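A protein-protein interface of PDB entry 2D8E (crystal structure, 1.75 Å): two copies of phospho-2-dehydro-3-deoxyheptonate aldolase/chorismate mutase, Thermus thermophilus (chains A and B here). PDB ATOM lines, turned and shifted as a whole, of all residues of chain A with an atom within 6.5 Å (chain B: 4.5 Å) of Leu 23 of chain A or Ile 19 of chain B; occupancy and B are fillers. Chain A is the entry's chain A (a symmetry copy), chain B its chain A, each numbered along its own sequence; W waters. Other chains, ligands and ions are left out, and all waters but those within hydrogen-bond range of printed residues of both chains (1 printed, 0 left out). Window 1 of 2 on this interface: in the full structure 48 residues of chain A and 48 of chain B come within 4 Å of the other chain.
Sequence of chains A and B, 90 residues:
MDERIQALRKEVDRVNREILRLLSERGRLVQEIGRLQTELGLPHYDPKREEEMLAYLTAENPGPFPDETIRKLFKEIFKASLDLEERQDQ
Glu 18 of chain A touches Leu 22 of chain B, and with the chains exchanged Leu 22 of chain A touches Glu 18 of chain B. Ile 19 of chain A touches Leu 22 of chain B, and with the chains exchanged Leu 22 of chain A touches Ile 19 of chain B. Ile 19 of chain A touches Phe 74 of chain B, and with the chains exchanged Phe 74 of chain A touches Ile 19 of chain B. Leu 20 of chain A touches Phe 74 of chain B, and with the chains exchanged Phe 74 of chain A touches Leu 20 of chain B. Of the 19 pairs that touch across the chains among the printed residues, 13 have their exchanged pair printed and touching as well.
OD1 of Asn 16 of chain B lies within hydrogen-bond range of NE of Arg 26 of chain A, 2.8 Å away.
The side-chain hydroxyl (OG) of Ser 24 of chain A sits at hydrogen-bond distance from the backbone carbonyl oxygen (O) of Leu 20 of chain A, 2.9 Å away.
Of the printed residues of chain B, Leu 23 of chain A touches Ile 19, Phe 65 and Phe 74. Glu 25 of chain A touches none of the printed residues of chain B. Of the printed residues of chain B, Phe 74 of chain A touches Asn 16 (3.5 Å), Ile 19 (3.7 Å), Leu 20 (3.9 Å) and Leu 23 (3.99 Å). Ile 19 of chain B touches just these residues of chain A: Leu 22, Leu 23 and Phe 74. Of the printed residues of chain A, Phe 65 of chain B touches Leu 23 (3.0 Å) and Gly 27 (3.8 Å). Leu 73 of chain B touches none of the printed residues of chain A. The nearest printed residue of chain B that does not touch Leu 23 of chain A is Leu 73 of chain B (4.3 Å). The nearest residue of chain A that does not touch Ile 19 of chain B is Arg 26 of chain A (4.3 Å). The nearest printed residue of chain B that does not touch Ile 19 of chain A is Ile 19 of chain B (5.0 Å).
Among the printed residues, pairs that only touch across the chains: Glu 18 of chain A with Leu 22 of chain B, Ile 19 of chain A with Leu 22 of chain B, Ile 19 of chain A with Leu 23 of chain B, Ile 19 of chain A with Phe 74 of chain B, Leu 20 of chain A with Phe 74 of chain B, Leu 22 of chain A with Val 15 of chain B, Leu 22 of chain A with Glu 18 of chain B, Leu 22 of chain A with Ile 19 of chain B, Leu 22 of chain A with Leu 22 of chain B, Leu 23 of chain A with Ile 19 of chain B, Leu 23 of chain A with Phe 65 of chain B, Leu 23 of chain A with Phe 74 of chain B, Arg 26 of chain A with Val 15 of chain B, Gly 27 of chain A with Phe 65 of chain B, Phe 74 of chain A with Asn 16 of chain B, Phe 74 of chain A with Ile 19 of chain B, Phe 74 of chain A with Leu 20 of chain B and Phe 74 of chain A with Leu 23 of chain B.
Hydrophobic or aromatic side chains of chain A within 4 Å of the printed part of chain B: Ile 19, Leu 22, Leu 23 and Phe 74. Of the 12 printed residues of chain B, 9 touch a printed residue of chain A. Among the printed residues, 19 pairs touch across the chains.
Water W1 lies within hydrogen-bond range of OG of Ser 24 of chain A (2.8 Å) and N of Phe 65 of chain B (3.2 Å).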
ATOM      1  N   GLU A  18      12.645   8.586  19.669  1.00  0.00           N
ATOM      2  CA  GLU A  18      11.592   8.775  20.660  1.00  0.00           C
ATOM      3  C   GLU A  18      10.531   9.688  20.054  1.00  0.00           C
ATOM      4  O   GLU A  18       9.333   9.458  20.205  1.00  0.00           O
ATOM      5  CB  GLU A  18      12.166   9.392  21.936  1.00  0.00           C
ATOM      6  CG  GLU A  18      13.184   8.503  22.633  1.00  0.00           C
ATOM      7  CD  GLU A  18      13.632   9.064  23.968  1.00  0.00           C
ATOM      8  OE1 GLU A  18      12.764   9.252  24.847  1.00  0.00           O
ATOM      9  OE2 GLU A  18      14.847   9.316  24.140  1.00  0.00           O
ATOM     10  N   ILE A  19      10.975  10.728  19.355  1.00  0.00           N
ATOM     11  CA  ILE A  19      10.039  11.648  18.719  1.00  0.00           C
ATOM     12  C   ILE A  19       9.217  10.923  17.660  1.00  0.00           C
ATOM     13  O   ILE A  19       8.017  11.156  17.524  1.00  0.00           O
ATOM     14  CB  ILE A  19      10.779  12.833  18.069  1.00  0.00           C
ATOM     15  CG1 ILE A  19      11.382  13.712  19.168  1.00  0.00           C
ATOM     16  CG2 ILE A  19       9.827  13.638  17.206  1.00  0.00           C
ATOM     17  CD1 ILE A  19      12.244  14.847  18.653  1.00  0.00           C
ATOM     18  N   LEU A  20       9.864  10.043  16.906  1.00  0.00           N
ATOM     19  CA  LEU A  20       9.151   9.287  15.885  1.00  0.00           C
ATOM     20  C   LEU A  20       8.064   8.449  16.551  1.00  0.00           C
ATOM     21  O   LEU A  20       6.948   8.362  16.045  1.00  0.00           O
ATOM     22  CB  LEU A  20      10.110   8.378  15.118  1.00  0.00           C
ATOM     23  CG  LEU A  20       9.456   7.413  14.122  1.00  0.00           C
ATOM     24  CD1 LEU A  20       8.657   8.166  13.069  1.00  0.00           C
ATOM     25  CD2 LEU A  20      10.535   6.579  13.479  1.00  0.00           C
ATOM     26  N   ARG A  21       8.381   7.842  17.692  1.00  0.00           N
ATOM     27  CA  ARG A  21       7.385   7.029  18.382  1.00  0.00           C
ATOM     28  C   ARG A  21       6.191   7.858  18.841  1.00  0.00           C
ATOM     29  O   ARG A  21       5.039   7.445  18.690  1.00  0.00           O
ATOM     30  CB  ARG A  21       7.967   6.324  19.611  1.00  0.00           C
ATOM     31  CG  ARG A  21       6.872   5.508  20.278  1.00  0.00           C
ATOM     32  CD  ARG A  21       7.219   4.813  21.570  1.00  0.00           C
ATOM     33  NE  ARG A  21       6.005   4.124  22.009  1.00  0.00           N
ATOM     34  CZ  ARG A  21       5.899   3.312  23.054  1.00  0.00           C
ATOM     35  NH1 ARG A  21       6.943   3.050  23.824  1.00  0.00           N
ATOM     36  NH2 ARG A  21       4.726   2.756  23.325  1.00  0.00           N
ATOM     37  N   LEU A  22       6.475   9.023  19.414  1.00  0.00           N
ATOM     38  CA  LEU A  22       5.425   9.904  19.898  1.00  0.00           C
ATOM     39  C   LEU A  22       4.590  10.443  18.750  1.00  0.00           C
ATOM     40  O   LEU A  22       3.374  10.561  18.872  1.00  0.00           O
ATOM     41  CB  LEU A  22       6.026  11.057  20.712  1.00  0.00           C
ATOM     42  CG  LEU A  22       6.260  10.784  22.199  1.00  0.00           C
ATOM     43  CD1 LEU A  22       7.092  11.807  22.974  1.00  0.00           C
ATOM     44  CD2 LEU A  22       4.947  10.629  22.968  1.00  0.00           C
ATOM     45  N   LEU A  23       5.234  10.776  17.635  1.00  0.00           N
ATOM     46  CA  LEU A  23       4.490  11.286  16.485  1.00  0.00           C
ATOM     47  C   LEU A  23       3.533  10.209  15.984  1.00  0.00           C
ATOM     48  O   LEU A  23       2.402  10.501  15.606  1.00  0.00           O
ATOM     49  CB  LEU A  23       5.440  11.697  15.351  1.00  0.00           C
ATOM     50  CG  LEU A  23       6.250  12.979  15.540  1.00  0.00           C
ATOM     51  CD1 LEU A  23       7.271  13.115  14.408  1.00  0.00           C
ATOM     52  CD2 LEU A  23       5.301  14.187  15.563  1.00  0.00           C
ATOM     53  N   SER A  24       3.994   8.962  15.986  1.00  0.00           N
ATOM     54  CA  SER A  24       3.171   7.849  15.530  1.00  0.00           C
ATOM     55  C   SER A  24       2.000   7.644  16.490  1.00  0.00           C
ATOM     56  O   SER A  24       0.870   7.380  16.067  1.00  0.00           O
ATOM     57  CB  SER A  24       4.021   6.584  15.424  1.00  0.00           C
ATOM     58  OG  SER A  24       5.062   6.771  14.477  1.00  0.00           O
ATOM     59  N   GLU A  25       2.277   7.773  17.783  1.00  0.00           N
ATOM     60  CA  GLU A  25       1.242   7.642  18.806  1.00  0.00           C
ATOM     61  C   GLU A  25       0.215   8.744  18.545  1.00  0.00           C
ATOM     62  O   GLU A  25      -0.995   8.504  18.549  1.00  0.00           O
ATOM     63  CB  GLU A  25       1.855   7.831  20.197  1.00  0.00           C
ATOM     64  CG  GLU A  25       0.854   7.762  21.337  1.00  0.00           C
ATOM     65  CD  GLU A  25       0.569   6.337  21.788  1.00  0.00           C
ATOM     66  OE1 GLU A  25       0.252   5.477  20.932  1.00  0.00           O
ATOM     67  OE2 GLU A  25       0.657   6.084  23.010  1.00  0.00           O
ATOM     68  N   ARG A  26       0.717   9.951  18.303  1.00  0.00           N
ATOM     69  CA  ARG A  26      -0.142  11.102  18.039  1.00  0.00           C
ATOM     70  C   ARG A  26      -0.991  10.863  16.791  1.00  0.00           C
ATOM     71  O   ARG A  26      -2.167  11.220  16.752  1.00  0.00           O
ATOM     72  CB  ARG A  26       0.704  12.364  17.845  1.00  0.00           C
ATOM     73  CG  ARG A  26      -0.104  13.659  17.929  1.00  0.00           C
ATOM     74  CD  ARG A  26       0.745  14.898  17.639  1.00  0.00           C
ATOM     75  NE  ARG A  26       0.036  16.122  18.015  1.00  0.00           N
ATOM     76  CZ  ARG A  26      -0.959  16.670  17.323  1.00  0.00           C
ATOM     77  NH1 ARG A  26      -1.380  16.120  16.191  1.00  0.00           N
ATOM     78  NH2 ARG A  26      -1.553  17.764  17.778  1.00  0.00           N
ATOM     79  N   GLY A  27      -0.383  10.268  15.770  1.00  0.00           N
ATOM     80  CA  GLY A  27      -1.107   9.994  14.543  1.00  0.00           C
ATOM     81  C   GLY A  27      -2.265   9.039  14.781  1.00  0.00           C
ATOM     82  O   GLY A  27      -3.355   9.221  14.239  1.00  0.00           O
ATOM     83  N   ARG A  28      -2.029   8.019  15.597  1.00  0.00           N
ATOM     84  CA  ARG A  28      -3.066   7.045  15.904  1.00  0.00           C
ATOM     85  C   ARG A  28      -4.223   7.723  16.623  1.00  0.00           C
ATOM     86  O   ARG A  28      -5.390   7.426  16.364  1.00  0.00           O
ATOM     87  CB  ARG A  28      -2.505   5.926  16.785  1.00  0.00           C
ATOM     88  CG  ARG A  28      -1.436   5.084  16.110  1.00  0.00           C
ATOM     89  CD  ARG A  28      -1.000   3.939  17.017  1.00  0.00           C
ATOM     90  NE  ARG A  28      -2.111   3.045  17.337  1.00  0.00           N
ATOM     91  CZ  ARG A  28      -2.039   2.034  18.199  1.00  0.00           C
ATOM     92  NH1 ARG A  28      -0.902   1.778  18.837  1.00  0.00           N
ATOM     93  NH2 ARG A  28      -3.103   1.277  18.424  1.00  0.00           N
ATOM     94  N   PHE A  74       5.058  22.875  15.759  1.00  0.00           N
ATOM     95  CA  PHE A  74       3.795  22.222  16.049  1.00  0.00           C
ATOM     96  C   PHE A  74       2.749  22.489  14.972  1.00  0.00           C
ATOM     97  O   PHE A  74       1.904  21.643  14.709  1.00  0.00           O
ATOM     98  CB  PHE A  74       3.307  22.604  17.443  1.00  0.00           C
ATOM     99  CG  PHE A  74       3.884  21.727  18.523  1.00  0.00           C
ATOM    100  CD1 PHE A  74       3.342  20.470  18.774  1.00  0.00           C
ATOM    101  CD2 PHE A  74       5.010  22.122  19.235  1.00  0.00           C
ATOM    102  CE1 PHE A  74       3.914  19.617  19.718  1.00  0.00           C
ATOM    103  CE2 PHE A  74       5.593  21.276  20.185  1.00  0.00           C
ATOM    104  CZ  PHE A  74       5.042  20.020  20.423  1.00  0.00           C
ATOM    105  N   ILE A  77       3.255  19.919  12.552  1.00  0.00           N
ATOM    106  CA  ILE A  77       2.736  18.654  13.048  1.00  0.00           C
ATOM    107  C   ILE A  77       1.213  18.609  12.884  1.00  0.00           C
ATOM    108  O   ILE A  77       0.649  17.577  12.500  1.00  0.00           O
ATOM    109  CB  ILE A  77       3.129  18.457  14.538  1.00  0.00           C
ATOM    110  CG1 ILE A  77       4.647  18.280  14.640  1.00  0.00           C
ATOM    111  CG2 ILE A  77       2.392  17.252  15.130  1.00  0.00           C
ATOM    112  CD1 ILE A  77       5.186  18.176  16.065  1.00  0.00           C
ATOM    113  N   VAL B  15       0.642  13.872  24.727  1.00  0.00           N
ATOM    114  CA  VAL B  15       1.639  13.566  23.706  1.00  0.00           C
ATOM    115  C   VAL B  15       2.333  14.842  23.233  1.00  0.00           C
ATOM    116  O   VAL B  15       3.550  14.854  23.031  1.00  0.00           O
ATOM    117  CB  VAL B  15       1.005  12.850  22.496  1.00  0.00           C
ATOM    118  CG1 VAL B  15       2.036  12.716  21.367  1.00  0.00           C
ATOM    119  CG2 VAL B  15       0.506  11.479  22.917  1.00  0.00           C
ATOM    120  N   ASN B  16       1.567  15.915  23.050  1.00  0.00           N
ATOM    121  CA  ASN B  16       2.156  17.183  22.621  1.00  0.00           C
ATOM    122  C   ASN B  16       3.227  17.634  23.601  1.00  0.00           C
ATOM    123  O   ASN B  16       4.308  18.065  23.199  1.00  0.00           O
ATOM    124  CB  ASN B  16       1.111  18.301  22.543  1.00  0.00           C
ATOM    125  CG  ASN B  16       0.263  18.234  21.292  1.00  0.00           C
ATOM    126  OD1 ASN B  16       0.592  17.535  20.330  1.00  0.00           O
ATOM    127  ND2 ASN B  16      -0.834  18.984  21.295  1.00  0.00           N
ATOM    128  N   ARG B  17       2.910  17.555  24.890  1.00  0.00           N
ATOM    129  CA  ARG B  17       3.843  17.970  25.929  1.00  0.00           C
ATOM    130  C   ARG B  17       5.087  17.089  25.963  1.00  0.00           C
ATOM    131  O   ARG B  17       6.188  17.568  26.229  1.00  0.00           O
ATOM    132  CB  ARG B  17       3.149  17.974  27.297  1.00  0.00           C
ATOM    133  CG  ARG B  17       2.051  19.028  27.402  1.00  0.00           C
ATOM    134  CD  ARG B  17       1.576  19.198  28.841  1.00  0.00           C
ATOM    135  NE  ARG B  17       0.755  20.392  29.019  1.00  0.00           N
ATOM    136  CZ  ARG B  17      -0.565  20.433  28.872  1.00  0.00           C
ATOM    137  NH1 ARG B  17      -1.235  19.338  28.540  1.00  0.00           N
ATOM    138  NH2 ARG B  17      -1.218  21.571  29.064  1.00  0.00           N
ATOM    139  N   GLU B  18       4.915  15.802  25.684  1.00  0.00           N
ATOM    140  CA  GLU B  18       6.058  14.896  25.668  1.00  0.00           C
ATOM    141  C   GLU B  18       6.956  15.288  24.499  1.00  0.00           C
ATOM    142  O   GLU B  18       8.179  15.320  24.618  1.00  0.00           O
ATOM    143  CB  GLU B  18       5.589  13.449  25.523  1.00  0.00           C
ATOM    144  CG  GLU B  18       4.743  12.966  26.692  1.00  0.00           C
ATOM    145  CD  GLU B  18       4.410  11.490  26.602  1.00  0.00           C
ATOM    146  OE1 GLU B  18       5.356  10.676  26.577  1.00  0.00           O
ATOM    147  OE2 GLU B  18       3.207  11.145  26.558  1.00  0.00           O
ATOM    148  N   ILE B  19       6.342  15.597  23.360  1.00  0.00           N
ATOM    149  CA  ILE B  19       7.112  16.005  22.190  1.00  0.00           C
ATOM    150  C   ILE B  19       7.861  17.301  22.471  1.00  0.00           C
ATOM    151  O   ILE B  19       9.012  17.465  22.067  1.00  0.00           O
ATOM    152  CB  ILE B  19       6.198  16.198  20.964  1.00  0.00           C
ATOM    153  CG1 ILE B  19       5.656  14.836  20.523  1.00  0.00           C
ATOM    154  CG2 ILE B  19       6.966  16.857  19.836  1.00  0.00           C
ATOM    155  CD1 ILE B  19       4.643  14.906  19.397  1.00  0.00           C
ATOM    156  N   LEU B  20       7.209  18.226  23.164  1.00  0.00           N
ATOM    157  CA  LEU B  20       7.859  19.486  23.498  1.00  0.00           C
ATOM    158  C   LEU B  20       9.086  19.204  24.358  1.00  0.00           C
ATOM    159  O   LEU B  20      10.138  19.808  24.161  1.00  0.00           O
ATOM    160  CB  LEU B  20       6.898  20.406  24.252  1.00  0.00           C
ATOM    161  CG  LEU B  20       7.511  21.701  24.799  1.00  0.00           C
ATOM    162  CD1 LEU B  20       8.110  22.542  23.682  1.00  0.00           C
ATOM    163  CD2 LEU B  20       6.441  22.469  25.532  1.00  0.00           C
ATOM    164  N   ARG B  21       8.962  18.277  25.305  1.00  0.00           N
ATOM    165  CA  ARG B  21      10.100  17.955  26.159  1.00  0.00           C
ATOM    166  C   ARG B  21      11.264  17.373  25.365  1.00  0.00           C
ATOM    167  O   ARG B  21      12.422  17.742  25.575  1.00  0.00           O
ATOM    168  CB  ARG B  21       9.733  16.951  27.256  1.00  0.00           C
ATOM    169  CG  ARG B  21      10.968  16.661  28.094  1.00  0.00           C
ATOM    170  CD  ARG B  21      10.839  15.615  29.172  1.00  0.00           C
ATOM    171  NE  ARG B  21      12.152  15.513  29.809  1.00  0.00           N
ATOM    172  CZ  ARG B  21      12.453  14.777  30.873  1.00  0.00           C
ATOM    173  NH1 ARG B  21      11.535  14.033  31.470  1.00  0.00           N
ATOM    174  NH2 ARG B  21      13.693  14.791  31.340  1.00  0.00           N
ATOM    175  N   LEU B  22      10.949  16.452  24.459  1.00  0.00           N
ATOM    176  CA  LEU B  22      11.968  15.818  23.639  1.00  0.00           C
ATOM    177  C   LEU B  22      12.609  16.818  22.693  1.00  0.00           C
ATOM    178  O   LEU B  22      13.817  16.772  22.473  1.00  0.00           O
ATOM    179  CB  LEU B  22      11.370  14.643  22.854  1.00  0.00           C
ATOM    180  CG  LEU B  22      11.339  13.294  23.575  1.00  0.00           C
ATOM    181  CD1 LEU B  22      10.520  12.177  22.929  1.00  0.00           C
ATOM    182  CD2 LEU B  22      12.743  12.727  23.790  1.00  0.00           C
ATOM    183  N   LEU B  23      11.811  17.719  22.129  1.00  0.00           N
ATOM    184  CA  LEU B  23      12.365  18.720  21.221  1.00  0.00           C
ATOM    185  C   LEU B  23      13.346  19.606  21.983  1.00  0.00           C
ATOM    186  O   LEU B  23      14.394  19.975  21.460  1.00  0.00           O
ATOM    187  CB  LEU B  23      11.254  19.589  20.613  1.00  0.00           C
ATOM    188  CG  LEU B  23      10.364  18.951  19.548  1.00  0.00           C
ATOM    189  CD1 LEU B  23       9.206  19.894  19.210  1.00  0.00           C
ATOM    190  CD2 LEU B  23      11.199  18.647  18.296  1.00  0.00           C
ATOM    191  N   PHE B  65       1.736   7.709   9.897  1.00  0.00           N
ATOM    192  CA  PHE B  65       2.266   8.719   8.986  1.00  0.00           C
ATOM    193  C   PHE B  65       3.086   8.052   7.889  1.00  0.00           C
ATOM    194  O   PHE B  65       3.805   7.091   8.143  1.00  0.00           O
ATOM    195  CB  PHE B  65       3.169   9.714   9.720  1.00  0.00           C
ATOM    196  CG  PHE B  65       2.434  10.687  10.590  1.00  0.00           C
ATOM    197  CD1 PHE B  65       2.516  10.600  11.975  1.00  0.00           C
ATOM    198  CD2 PHE B  65       1.673  11.708  10.026  1.00  0.00           C
ATOM    199  CE1 PHE B  65       1.856  11.516  12.786  1.00  0.00           C
ATOM    200  CE2 PHE B  65       1.009  12.630  10.831  1.00  0.00           C
ATOM    201  CZ  PHE B  65       1.102  12.533  12.214  1.00  0.00           C
ATOM    202  N   LEU B  73       8.562  16.309   8.321  1.00  0.00           N
ATOM    203  CA  LEU B  73       8.498  16.791   9.691  1.00  0.00           C
ATOM    204  C   LEU B  73       9.889  16.879  10.294  1.00  0.00           C
ATOM    205  O   LEU B  73      10.233  17.869  10.941  1.00  0.00           O
ATOM    206  CB  LEU B  73       7.617  15.870  10.541  1.00  0.00           C
ATOM    207  CG  LEU B  73       6.119  15.981  10.247  1.00  0.00           C
ATOM    208  CD1 LEU B  73       5.353  14.951  11.057  1.00  0.00           C
ATOM    209  CD2 LEU B  73       5.642  17.390  10.573  1.00  0.00           C
ATOM    210  N   PHE B  74      10.702  15.852  10.078  1.00  0.00           N
ATOM    211  CA  PHE B  74      12.043  15.885  10.631  1.00  0.00           C
ATOM    212  C   PHE B  74      12.925  16.917   9.939  1.00  0.00           C
ATOM    213  O   PHE B  74      13.804  17.498  10.565  1.00  0.00           O
ATOM    214  CB  PHE B  74      12.658  14.489  10.618  1.00  0.00           C
ATOM    215  CG  PHE B  74      12.292  13.679  11.834  1.00  0.00           C
ATOM    216  CD1 PHE B  74      12.969  13.869  13.035  1.00  0.00           C
ATOM    217  CD2 PHE B  74      11.229  12.785  11.801  1.00  0.00           C
ATOM    218  CE1 PHE B  74      12.590  13.181  14.188  1.00  0.00           C
ATOM    219  CE2 PHE B  74      10.840  12.089  12.950  1.00  0.00           C
ATOM    220  CZ  PHE B  74      11.523  12.291  14.146  1.00  0.00           C
HETATM  221  O   HOH W   1       4.206   7.400  11.859  1.00  0.00           O
